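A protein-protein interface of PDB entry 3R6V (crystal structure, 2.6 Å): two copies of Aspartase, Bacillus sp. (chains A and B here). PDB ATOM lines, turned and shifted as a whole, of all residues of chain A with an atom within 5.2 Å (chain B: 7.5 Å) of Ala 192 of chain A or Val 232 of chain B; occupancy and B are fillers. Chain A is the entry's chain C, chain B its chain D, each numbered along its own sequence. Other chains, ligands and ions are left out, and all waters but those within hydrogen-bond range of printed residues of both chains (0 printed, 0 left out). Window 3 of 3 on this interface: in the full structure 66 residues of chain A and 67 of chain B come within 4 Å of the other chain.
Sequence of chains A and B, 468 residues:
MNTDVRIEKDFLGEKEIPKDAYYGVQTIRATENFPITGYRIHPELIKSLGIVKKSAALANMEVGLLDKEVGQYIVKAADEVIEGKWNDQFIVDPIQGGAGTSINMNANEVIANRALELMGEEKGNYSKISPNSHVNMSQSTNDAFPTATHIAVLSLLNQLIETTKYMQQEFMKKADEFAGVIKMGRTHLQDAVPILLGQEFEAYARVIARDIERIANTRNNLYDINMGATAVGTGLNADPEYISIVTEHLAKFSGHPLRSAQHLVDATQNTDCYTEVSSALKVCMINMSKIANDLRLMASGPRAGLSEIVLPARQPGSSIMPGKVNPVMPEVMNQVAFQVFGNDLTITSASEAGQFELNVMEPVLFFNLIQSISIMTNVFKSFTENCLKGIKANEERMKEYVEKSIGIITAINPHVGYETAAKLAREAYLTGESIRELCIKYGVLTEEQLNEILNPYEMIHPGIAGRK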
ATOM      1  N   MET A 184      -5.123   4.077  20.300  1.00  0.00           N
ATOM      2  CA  MET A 184      -5.662   2.829  20.813  1.00  0.00           C
ATOM      3  C   MET A 184      -5.190   2.613  22.235  1.00  0.00           C
ATOM      4  O   MET A 184      -3.984   2.631  22.511  1.00  0.00           O
ATOM      5  CB  MET A 184      -5.282   1.632  19.927  1.00  0.00           C
ATOM      6  CG  MET A 184      -6.203   1.414  18.751  1.00  0.00           C
ATOM      7  SD  MET A 184      -7.947   1.279  19.227  1.00  0.00           S
ATOM      8  CE  MET A 184      -8.525   2.926  18.958  1.00  0.00           C
ATOM      9  N   GLY A 185      -6.146   2.417  23.136  1.00  0.00           N
ATOM     10  CA  GLY A 185      -5.821   1.940  24.471  1.00  0.00           C
ATOM     11  C   GLY A 185      -5.440   0.480  24.370  1.00  0.00           C
ATOM     12  O   GLY A 185      -5.898  -0.221  23.464  1.00  0.00           O
ATOM     13  N   ARG A 186      -4.597   0.021  25.291  1.00  0.00           N
ATOM     14  CA  ARG A 186      -4.146  -1.367  25.293  1.00  0.00           C
ATOM     15  C   ARG A 186      -4.318  -1.976  26.675  1.00  0.00           C
ATOM     16  O   ARG A 186      -4.034  -1.321  27.677  1.00  0.00           O
ATOM     17  CB  ARG A 186      -2.673  -1.447  24.889  1.00  0.00           C
ATOM     18  CG  ARG A 186      -2.353  -1.063  23.459  1.00  0.00           C
ATOM     19  CD  ARG A 186      -0.848  -1.123  23.264  1.00  0.00           C
ATOM     20  NE  ARG A 186      -0.417  -0.633  21.964  1.00  0.00           N
ATOM     21  CZ  ARG A 186      -0.237   0.646  21.662  1.00  0.00           C
ATOM     22  NH1 ARG A 186      -0.463   1.592  22.558  1.00  0.00           N
ATOM     23  NH2 ARG A 186       0.163   0.982  20.451  1.00  0.00           N
ATOM     24  N   THR A 187      -4.792  -3.224  26.725  1.00  0.00           N
ATOM     25  CA  THR A 187      -4.838  -4.011  27.982  1.00  0.00           C
ATOM     26  C   THR A 187      -4.309  -5.426  27.759  1.00  0.00           C
ATOM     27  O   THR A 187      -4.680  -6.099  26.791  1.00  0.00           O
ATOM     28  CB  THR A 187      -6.240  -4.062  28.637  1.00  0.00           C
ATOM     29  OG1 THR A 187      -7.157  -4.785  27.808  1.00  0.00           O
ATOM     30  CG2 THR A 187      -6.777  -2.659  28.886  1.00  0.00           C
ATOM     31  N   GLN A 190      -2.663  -5.989  24.525  1.00  0.00           N
ATOM     32  CA  GLN A 190      -3.493  -6.393  23.423  1.00  0.00           C
ATOM     33  C   GLN A 190      -4.412  -5.187  23.161  1.00  0.00           C
ATOM     34  O   GLN A 190      -4.963  -4.627  24.115  1.00  0.00           O
ATOM     35  CB  GLN A 190      -4.257  -7.651  23.880  1.00  0.00           C
ATOM     36  CG  GLN A 190      -4.695  -8.631  22.792  1.00  0.00           C
ATOM     37  CD  GLN A 190      -3.573  -9.483  22.194  1.00  0.00           C
ATOM     38  OE1 GLN A 190      -2.440  -9.512  22.687  1.00  0.00           O
ATOM     39  NE2 GLN A 190      -3.902 -10.195  21.111  1.00  0.00           N
ATOM     40  N   ASP A 191      -4.530  -4.740  21.905  1.00  0.00           N
ATOM     41  CA  ASP A 191      -5.447  -3.626  21.526  1.00  0.00           C
ATOM     42  C   ASP A 191      -6.776  -3.671  22.283  1.00  0.00           C
ATOM     43  O   ASP A 191      -7.396  -4.732  22.384  1.00  0.00           O
ATOM     44  CB  ASP A 191      -5.833  -3.663  20.035  1.00  0.00           C
ATOM     45  CG  ASP A 191      -4.652  -3.751  19.095  1.00  0.00           C
ATOM     46  OD1 ASP A 191      -4.891  -4.162  17.939  1.00  0.00           O
ATOM     47  OD2 ASP A 191      -3.505  -3.423  19.481  1.00  0.00           O
ATOM     48  N   ALA A 192      -7.242  -2.531  22.777  1.00  0.00           N
ATOM     49  CA  ALA A 192      -8.538  -2.508  23.459  1.00  0.00           C
ATOM     50  C   ALA A 192      -9.534  -1.627  22.731  1.00  0.00           C
ATOM     51  O   ALA A 192     -10.043  -1.988  21.671  1.00  0.00           O
ATOM     52  CB  ALA A 192      -8.390  -2.071  24.915  1.00  0.00           C
ATOM     53  N   VAL A 193      -9.809  -0.472  23.325  1.00  0.00           N
ATOM     54  CA  VAL A 193     -10.741   0.494  22.776  1.00  0.00           C
ATOM     55  C   VAL A 193     -10.035   1.828  22.792  1.00  0.00           C
ATOM     56  O   VAL A 193      -9.019   1.968  23.463  1.00  0.00           O
ATOM     57  CB  VAL A 193     -12.059   0.561  23.593  1.00  0.00           C
ATOM     58  CG1 VAL A 193     -12.863  -0.702  23.382  1.00  0.00           C
ATOM     59  CG2 VAL A 193     -11.786   0.786  25.083  1.00  0.00           C
ATOM     60  N   PRO A 194     -10.550   2.806  22.028  1.00  0.00           N
ATOM     61  CA  PRO A 194      -9.945   4.136  21.981  1.00  0.00           C
ATOM     62  C   PRO A 194      -9.676   4.756  23.348  1.00  0.00           C
ATOM     63  O   PRO A 194     -10.491   4.636  24.274  1.00  0.00           O
ATOM     64  CB  PRO A 194     -10.992   4.953  21.236  1.00  0.00           C
ATOM     65  CG  PRO A 194     -11.575   3.967  20.268  1.00  0.00           C
ATOM     66  CD  PRO A 194     -11.548   2.628  20.955  1.00  0.00           C
ATOM     67  N   ILE A 195      -8.520   5.397  23.453  1.00  0.00           N
ATOM     68  CA  ILE A 195      -8.217   6.273  24.556  1.00  0.00           C
ATOM     69  C   ILE A 195      -7.564   7.537  23.997  1.00  0.00           C
ATOM     70  O   ILE A 195      -7.085   7.547  22.871  1.00  0.00           O
ATOM     71  CB  ILE A 195      -7.308   5.566  25.599  1.00  0.00           C
ATOM     72  CG1 ILE A 195      -7.564   6.134  27.003  1.00  0.00           C
ATOM     73  CG2 ILE A 195      -5.817   5.586  25.168  1.00  0.00           C
ATOM     74  CD1 ILE A 195      -6.636   5.615  28.079  1.00  0.00           C
ATOM     75  N   GLY A 407     -11.231  -2.489  17.678  1.00  0.00           N
ATOM     76  CA  GLY A 407     -11.834  -1.935  18.887  1.00  0.00           C
ATOM     77  C   GLY A 407     -12.913  -0.891  18.703  1.00  0.00           C
ATOM     78  O   GLY A 407     -13.819  -0.770  19.538  1.00  0.00           O
ATOM     79  N   SER B 140     -16.832  -4.546  33.555  1.00  0.00           N
ATOM     80  CA  SER B 140     -15.682  -5.165  32.961  1.00  0.00           C
ATOM     81  C   SER B 140     -15.020  -5.977  34.063  1.00  0.00           C
ATOM     82  O   SER B 140     -15.387  -5.840  35.231  1.00  0.00           O
ATOM     83  CB  SER B 140     -14.735  -4.075  32.484  1.00  0.00           C
ATOM     84  OG  SER B 140     -13.742  -4.607  31.650  1.00  0.00           O
ATOM     85  N   ASN B 142     -12.134  -5.173  34.653  1.00  0.00           N
ATOM     86  CA  ASN B 142     -11.217  -4.105  35.054  1.00  0.00           C
ATOM     87  C   ASN B 142     -11.804  -3.036  35.985  1.00  0.00           C
ATOM     88  O   ASN B 142     -11.124  -2.064  36.337  1.00  0.00           O
ATOM     89  CB  ASN B 142     -10.607  -3.458  33.797  1.00  0.00           C
ATOM     90  CG  ASN B 142      -9.848  -4.458  32.926  1.00  0.00           C
ATOM     91  OD1 ASN B 142      -9.714  -5.626  33.284  1.00  0.00           O
ATOM     92  ND2 ASN B 142      -9.337  -3.999  31.788  1.00  0.00           N
ATOM     93  N   ASN B 226     -13.369   2.664  40.805  1.00  0.00           N
ATOM     94  CA  ASN B 226     -13.459   2.940  39.359  1.00  0.00           C
ATOM     95  C   ASN B 226     -14.667   2.291  38.672  1.00  0.00           C
ATOM     96  O   ASN B 226     -14.674   2.086  37.468  1.00  0.00           O
ATOM     97  CB  ASN B 226     -12.151   2.548  38.646  1.00  0.00           C
ATOM     98  CG  ASN B 226     -12.035   1.053  38.400  1.00  0.00           C
ATOM     99  OD1 ASN B 226     -12.517   0.240  39.191  1.00  0.00           O
ATOM    100  ND2 ASN B 226     -11.391   0.680  37.289  1.00  0.00           N
ATOM    101  N   ALA B 229     -16.031   2.382  34.754  1.00  0.00           N
ATOM    102  CA  ALA B 229     -14.912   2.699  33.880  1.00  0.00           C
ATOM    103  C   ALA B 229     -14.938   1.848  32.624  1.00  0.00           C
ATOM    104  O   ALA B 229     -14.431   2.257  31.568  1.00  0.00           O
ATOM    105  CB  ALA B 229     -13.619   2.468  34.627  1.00  0.00           C
ATOM    106  N   THR B 230     -15.547   0.670  32.746  1.00  0.00           N
ATOM    107  CA  THR B 230     -15.515  -0.373  31.708  1.00  0.00           C
ATOM    108  C   THR B 230     -14.079  -0.817  31.381  1.00  0.00           C
ATOM    109  O   THR B 230     -13.289  -1.069  32.290  1.00  0.00           O
ATOM    110  CB  THR B 230     -16.388  -0.054  30.426  1.00  0.00           C
ATOM    111  OG1 THR B 230     -15.904   1.110  29.735  1.00  0.00           O
ATOM    112  CG2 THR B 230     -17.853   0.131  30.819  1.00  0.00           C
ATOM    113  N   ALA B 231     -13.742  -0.914  30.103  1.00  0.00           N
ATOM    114  CA  ALA B 231     -12.523  -1.617  29.724  1.00  0.00           C
ATOM    115  C   ALA B 231     -11.247  -0.923  30.192  1.00  0.00           C
ATOM    116  O   ALA B 231     -10.384  -1.543  30.799  1.00  0.00           O
ATOM    117  CB  ALA B 231     -12.490  -1.856  28.208  1.00  0.00           C
ATOM    118  N   VAL B 232     -11.167   0.375  29.941  1.00  0.00           N
ATOM    119  CA  VAL B 232      -9.914   1.106  29.983  1.00  0.00           C
ATOM    120  C   VAL B 232     -10.034   2.332  30.883  1.00  0.00           C
ATOM    121  O   VAL B 232      -9.039   3.024  31.155  1.00  0.00           O
ATOM    122  CB  VAL B 232      -9.539   1.510  28.544  1.00  0.00           C
ATOM    123  CG1 VAL B 232      -8.864   2.858  28.487  1.00  0.00           C
ATOM    124  CG2 VAL B 232      -8.710   0.423  27.892  1.00  0.00           C
ATOM    125  N   GLY B 233     -11.256   2.574  31.362  1.00  0.00           N
ATOM    126  CA  GLY B 233     -11.586   3.768  32.126  1.00  0.00           C
ATOM    127  C   GLY B 233     -12.274   4.859  31.317  1.00  0.00           C
ATOM    128  O   GLY B 233     -12.463   5.973  31.821  1.00  0.00           O
ATOM    129  N   THR B 234     -12.629   4.568  30.063  1.00  0.00           N
ATOM    130  CA  THR B 234     -13.294   5.577  29.232  1.00  0.00           C
ATOM    131  C   THR B 234     -14.778   5.632  29.542  1.00  0.00           C
ATOM    132  O   THR B 234     -15.395   6.667  29.419  1.00  0.00           O
ATOM    133  CB  THR B 234     -13.044   5.437  27.684  1.00  0.00           C
ATOM    134  OG1 THR B 234     -13.479   4.165  27.203  1.00  0.00           O
ATOM    135  CG2 THR B 234     -11.577   5.643  27.326  1.00  0.00           C
ATOM    136  N   GLY B 235     -15.339   4.509  29.975  1.00  0.00           N
ATOM    137  CA  GLY B 235     -16.765   4.444  30.277  1.00  0.00           C
ATOM    138  C   GLY B 235     -17.584   4.503  28.999  1.00  0.00           C
ATOM    139  O   GLY B 235     -18.753   4.892  29.024  1.00  0.00           O
ATOM    140  N   LEU B 236     -16.954   4.119  27.884  1.00  0.00           N
ATOM    141  CA  LEU B 236     -17.617   3.962  26.586  1.00  0.00           C
ATOM    142  C   LEU B 236     -18.971   3.250  26.716  1.00  0.00           C
ATOM    143  O   LEU B 236     -19.044   2.098  27.154  1.00  0.00           O
ATOM    144  CB  LEU B 236     -16.701   3.209  25.607  1.00  0.00           C
ATOM    145  CG  LEU B 236     -17.103   3.096  24.131  1.00  0.00           C
ATOM    146  CD1 LEU B 236     -17.782   4.370  23.601  1.00  0.00           C
ATOM    147  CD2 LEU B 236     -15.890   2.730  23.275  1.00  0.00           C
ATOM    148  N   LEU B 264     -11.303   8.372  35.901  1.00  0.00           N
ATOM    149  CA  LEU B 264     -11.531   6.937  35.831  1.00  0.00           C
ATOM    150  C   LEU B 264     -10.414   6.159  35.177  1.00  0.00           C
ATOM    151  O   LEU B 264     -10.121   5.035  35.591  1.00  0.00           O
ATOM    152  CB  LEU B 264     -12.857   6.641  35.149  1.00  0.00           C
ATOM    153  CG  LEU B 264     -13.980   6.148  36.076  1.00  0.00           C
ATOM    154  CD1 LEU B 264     -13.948   6.777  37.471  1.00  0.00           C
ATOM    155  CD2 LEU B 264     -15.342   6.352  35.424  1.00  0.00           C
ATOM    156  N   VAL B 265      -9.792   6.760  34.167  1.00  0.00           N
ATOM    157  CA  VAL B 265      -8.658   6.158  33.489  1.00  0.00           C
ATOM    158  C   VAL B 265      -7.533   5.988  34.516  1.00  0.00           C
ATOM    159  O   VAL B 265      -7.007   4.888  34.693  1.00  0.00           O
ATOM    160  CB  VAL B 265      -8.209   7.011  32.255  1.00  0.00           C
ATOM    161  CG1 VAL B 265      -6.800   6.646  31.793  1.00  0.00           C
ATOM    162  CG2 VAL B 265      -9.202   6.881  31.105  1.00  0.00           C
ATOM    163  N   ASP B 266      -7.196   7.080  35.203  1.00  0.00           N
ATOM    164  CA  ASP B 266      -6.236   7.063  36.311  1.00  0.00           C
ATOM    165  C   ASP B 266      -6.538   5.938  37.296  1.00  0.00           C
ATOM    166  O   ASP B 266      -5.663   5.121  37.607  1.00  0.00           O
ATOM    167  CB  ASP B 266      -6.234   8.410  37.034  1.00  0.00           C
ATOM    168  CG  ASP B 266      -5.579   8.344  38.401  1.00  0.00           C
ATOM    169  OD1 ASP B 266      -4.483   7.744  38.513  1.00  0.00           O
ATOM    170  OD2 ASP B 266      -6.158   8.903  39.364  1.00  0.00           O
ATOM    171  N   ALA B 267      -7.779   5.880  37.770  1.00  0.00           N
ATOM    172  CA  ALA B 267      -8.176   4.835  38.707  1.00  0.00           C
ATOM    173  C   ALA B 267      -8.062   3.423  38.115  1.00  0.00           C
ATOM    174  O   ALA B 267      -7.834   2.469  38.851  1.00  0.00           O
ATOM    175  CB  ALA B 267      -9.581   5.089  39.211  1.00  0.00           C
ATOM    176  N   THR B 268      -8.211   3.296  36.793  1.00  0.00           N
ATOM    177  CA  THR B 268      -8.216   1.992  36.128  1.00  0.00           C
ATOM    178  C   THR B 268      -6.814   1.405  35.938  1.00  0.00           C
ATOM    179  O   THR B 268      -6.646   0.180  35.974  1.00  0.00           O
ATOM    180  CB  THR B 268      -8.922   2.080  34.768  1.00  0.00           C
ATOM    181  OG1 THR B 268     -10.273   2.502  34.974  1.00  0.00           O
ATOM    182  CG2 THR B 268      -8.923   0.734  34.017  1.00  0.00           C
ATOM    183  N   GLN B 269      -5.821   2.273  35.742  1.00  0.00           N
ATOM    184  CA  GLN B 269      -4.458   1.840  35.408  1.00  0.00           C
ATOM    185  C   GLN B 269      -3.395   2.002  36.515  1.00  0.00           C
ATOM    186  O   GLN B 269      -2.335   1.380  36.446  1.00  0.00           O
ATOM    187  CB  GLN B 269      -3.980   2.489  34.095  1.00  0.00           C
ATOM    188  CG  GLN B 269      -3.727   4.007  34.127  1.00  0.00           C
ATOM    189  CD  GLN B 269      -3.174   4.532  32.800  1.00  0.00           C
ATOM    190  OE1 GLN B 269      -2.023   4.972  32.722  1.00  0.00           O
ATOM    191  NE2 GLN B 269      -3.987   4.467  31.747  1.00  0.00           N
ATOM    192  N   PHE B 356       0.493   0.441  30.259  1.00  0.00           N
ATOM    193  CA  PHE B 356      -0.608   1.180  29.644  1.00  0.00           C
ATOM    194  C   PHE B 356      -1.843   1.153  30.534  1.00  0.00           C
ATOM    195  O   PHE B 356      -1.764   1.536  31.708  1.00  0.00           O
ATOM    196  CB  PHE B 356      -0.899   0.682  28.225  1.00  0.00           C
ATOM    197  CG  PHE B 356       0.173   1.034  27.229  1.00  0.00           C
ATOM    198  CD1 PHE B 356       0.474   2.368  26.941  1.00  0.00           C
ATOM    199  CD2 PHE B 356       0.872   0.039  26.563  1.00  0.00           C
ATOM    200  CE1 PHE B 356       1.458   2.696  26.018  1.00  0.00           C
ATOM    201  CE2 PHE B 356       1.858   0.359  25.637  1.00  0.00           C
ATOM    202  CZ  PHE B 356       2.149   1.691  25.367  1.00  0.00           C
ATOM    203  N   GLU B 357      -2.977   0.763  29.975  1.00  0.00           N
ATOM    204  CA  GLU B 357      -4.267   0.985  30.621  1.00  0.00           C
ATOM    205  C   GLU B 357      -4.593   0.004  31.753  1.00  0.00           C
ATOM    206  O   GLU B 357      -5.552   0.233  32.485  1.00  0.00           O
ATOM    207  CB  GLU B 357      -5.386   0.968  29.575  1.00  0.00           C
ATOM    208  CG  GLU B 357      -5.571   2.279  28.822  1.00  0.00           C
ATOM    209  CD  GLU B 357      -4.308   2.784  28.140  1.00  0.00           C
ATOM    210  OE1 GLU B 357      -3.720   3.773  28.627  1.00  0.00           O
ATOM    211  OE2 GLU B 357      -3.898   2.190  27.122  1.00  0.00           O
ATOM    212  N   LEU B 358      -3.819  -1.071  31.911  1.00  0.00           N
ATOM    213  CA  LEU B 358      -4.124  -2.063  32.942  1.00  0.00           C
ATOM    214  C   LEU B 358      -2.881  -2.746  33.507  1.00  0.00           C
ATOM    215  O   LEU B 358      -1.972  -3.105  32.765  1.00  0.00           O
ATOM    216  CB  LEU B 358      -5.074  -3.127  32.381  1.00  0.00           C
ATOM    217  CG  LEU B 358      -5.580  -4.231  33.317  1.00  0.00           C
ATOM    218  CD1 LEU B 358      -6.647  -3.703  34.277  1.00  0.00           C
ATOM    219  CD2 LEU B 358      -6.125  -5.380  32.519  1.00  0.00           C
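N of Ala 192 of chain A sits at hydrogen-bond distance from O of Gly 185 of chain A (2.8 Å). O of Val 193 of chain A lies within hydrogen-bond range of N of Gly 185 of chain A (2.9 Å). N of Thr 234 of chain B sits at hydrogen-bond distance from O of Ala 229 of chain B (3.3 Å). NE2 of Gln 269 of chain B is in hydrogen-bond range of OE1 of Glu 357 of chain B (3.2 Å).
The backbone NH (N) of Arg 186 of chain A is in hydrogen-bond range of the side-chain carboxylate (OE2) of Glu 357 of chain B, 2.9 Å away.
No position is printed for both chains.
Ala 192 of chain A touches one residue of chain B. Printed residues of chain A within 4 Å of Val 232 of chain B: Thr 187, Ala 192 and Ile 195. Of the printed residues of chain A, Glu 357 of chain B touches Gly 185, Arg 186, Thr 187 and Ile 195. Of the printed residues of chain A, Val 265 of chain B touches Ile 195. Of the printed residues of chain B, Arg 186 of chain A touches Phe 356 (3.8 Å) and Glu 357 (2.9 Å). Of the printed residues of chain B, Thr 187 of chain A touches Val 232, Glu 357 and Leu 358. Printed residues of chain A within 4 Å of Thr 234 of chain B: Pro 194. The nearest residue of chain B that does not touch Ala 192 of chain A is Ala 231 of chain B (5.3 Å).
Of the 20 printed residues of chain B, 6 touch a printed residue of chain A. Of the 11 printed residues of chain A, 6 touch a printed residue of chain B. Printed residues of chain A that touch a printed residue of chain B: Gly 185, Arg 186, Thr 187, Ala 192, Pro 194 and Ile 195. Among the printed residues, 11 pairs touch across the chains.
Gly 185 of chain A touches Glu 357 of chain B. O of Arg 186 of chain A touches CB of Phe 356 of chain B, 3.8 Å away. Thr 187 of chain A touches Val 232 of chain B. Glu 357 of chain B touches Thr 187 of chain A. CB of Leu 358 of chain B touches CG2 of Thr 187 of chain A (3.9 Å). Ala 192 of chain A touches Val 232 of chain B (CB to CG2, 3.9 Å). Pro 194 of chain A touches Thr 234 of chain B. CD1 of Ile 195 of chain A touches CG1 of Val 232 of chain B, at 3.6 Å. Ile 195 of chain A touches Val 265 of chain B (CD1 to CG1, 3.9 Å). Ile 195 of chain A touches Glu 357 of chain B.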
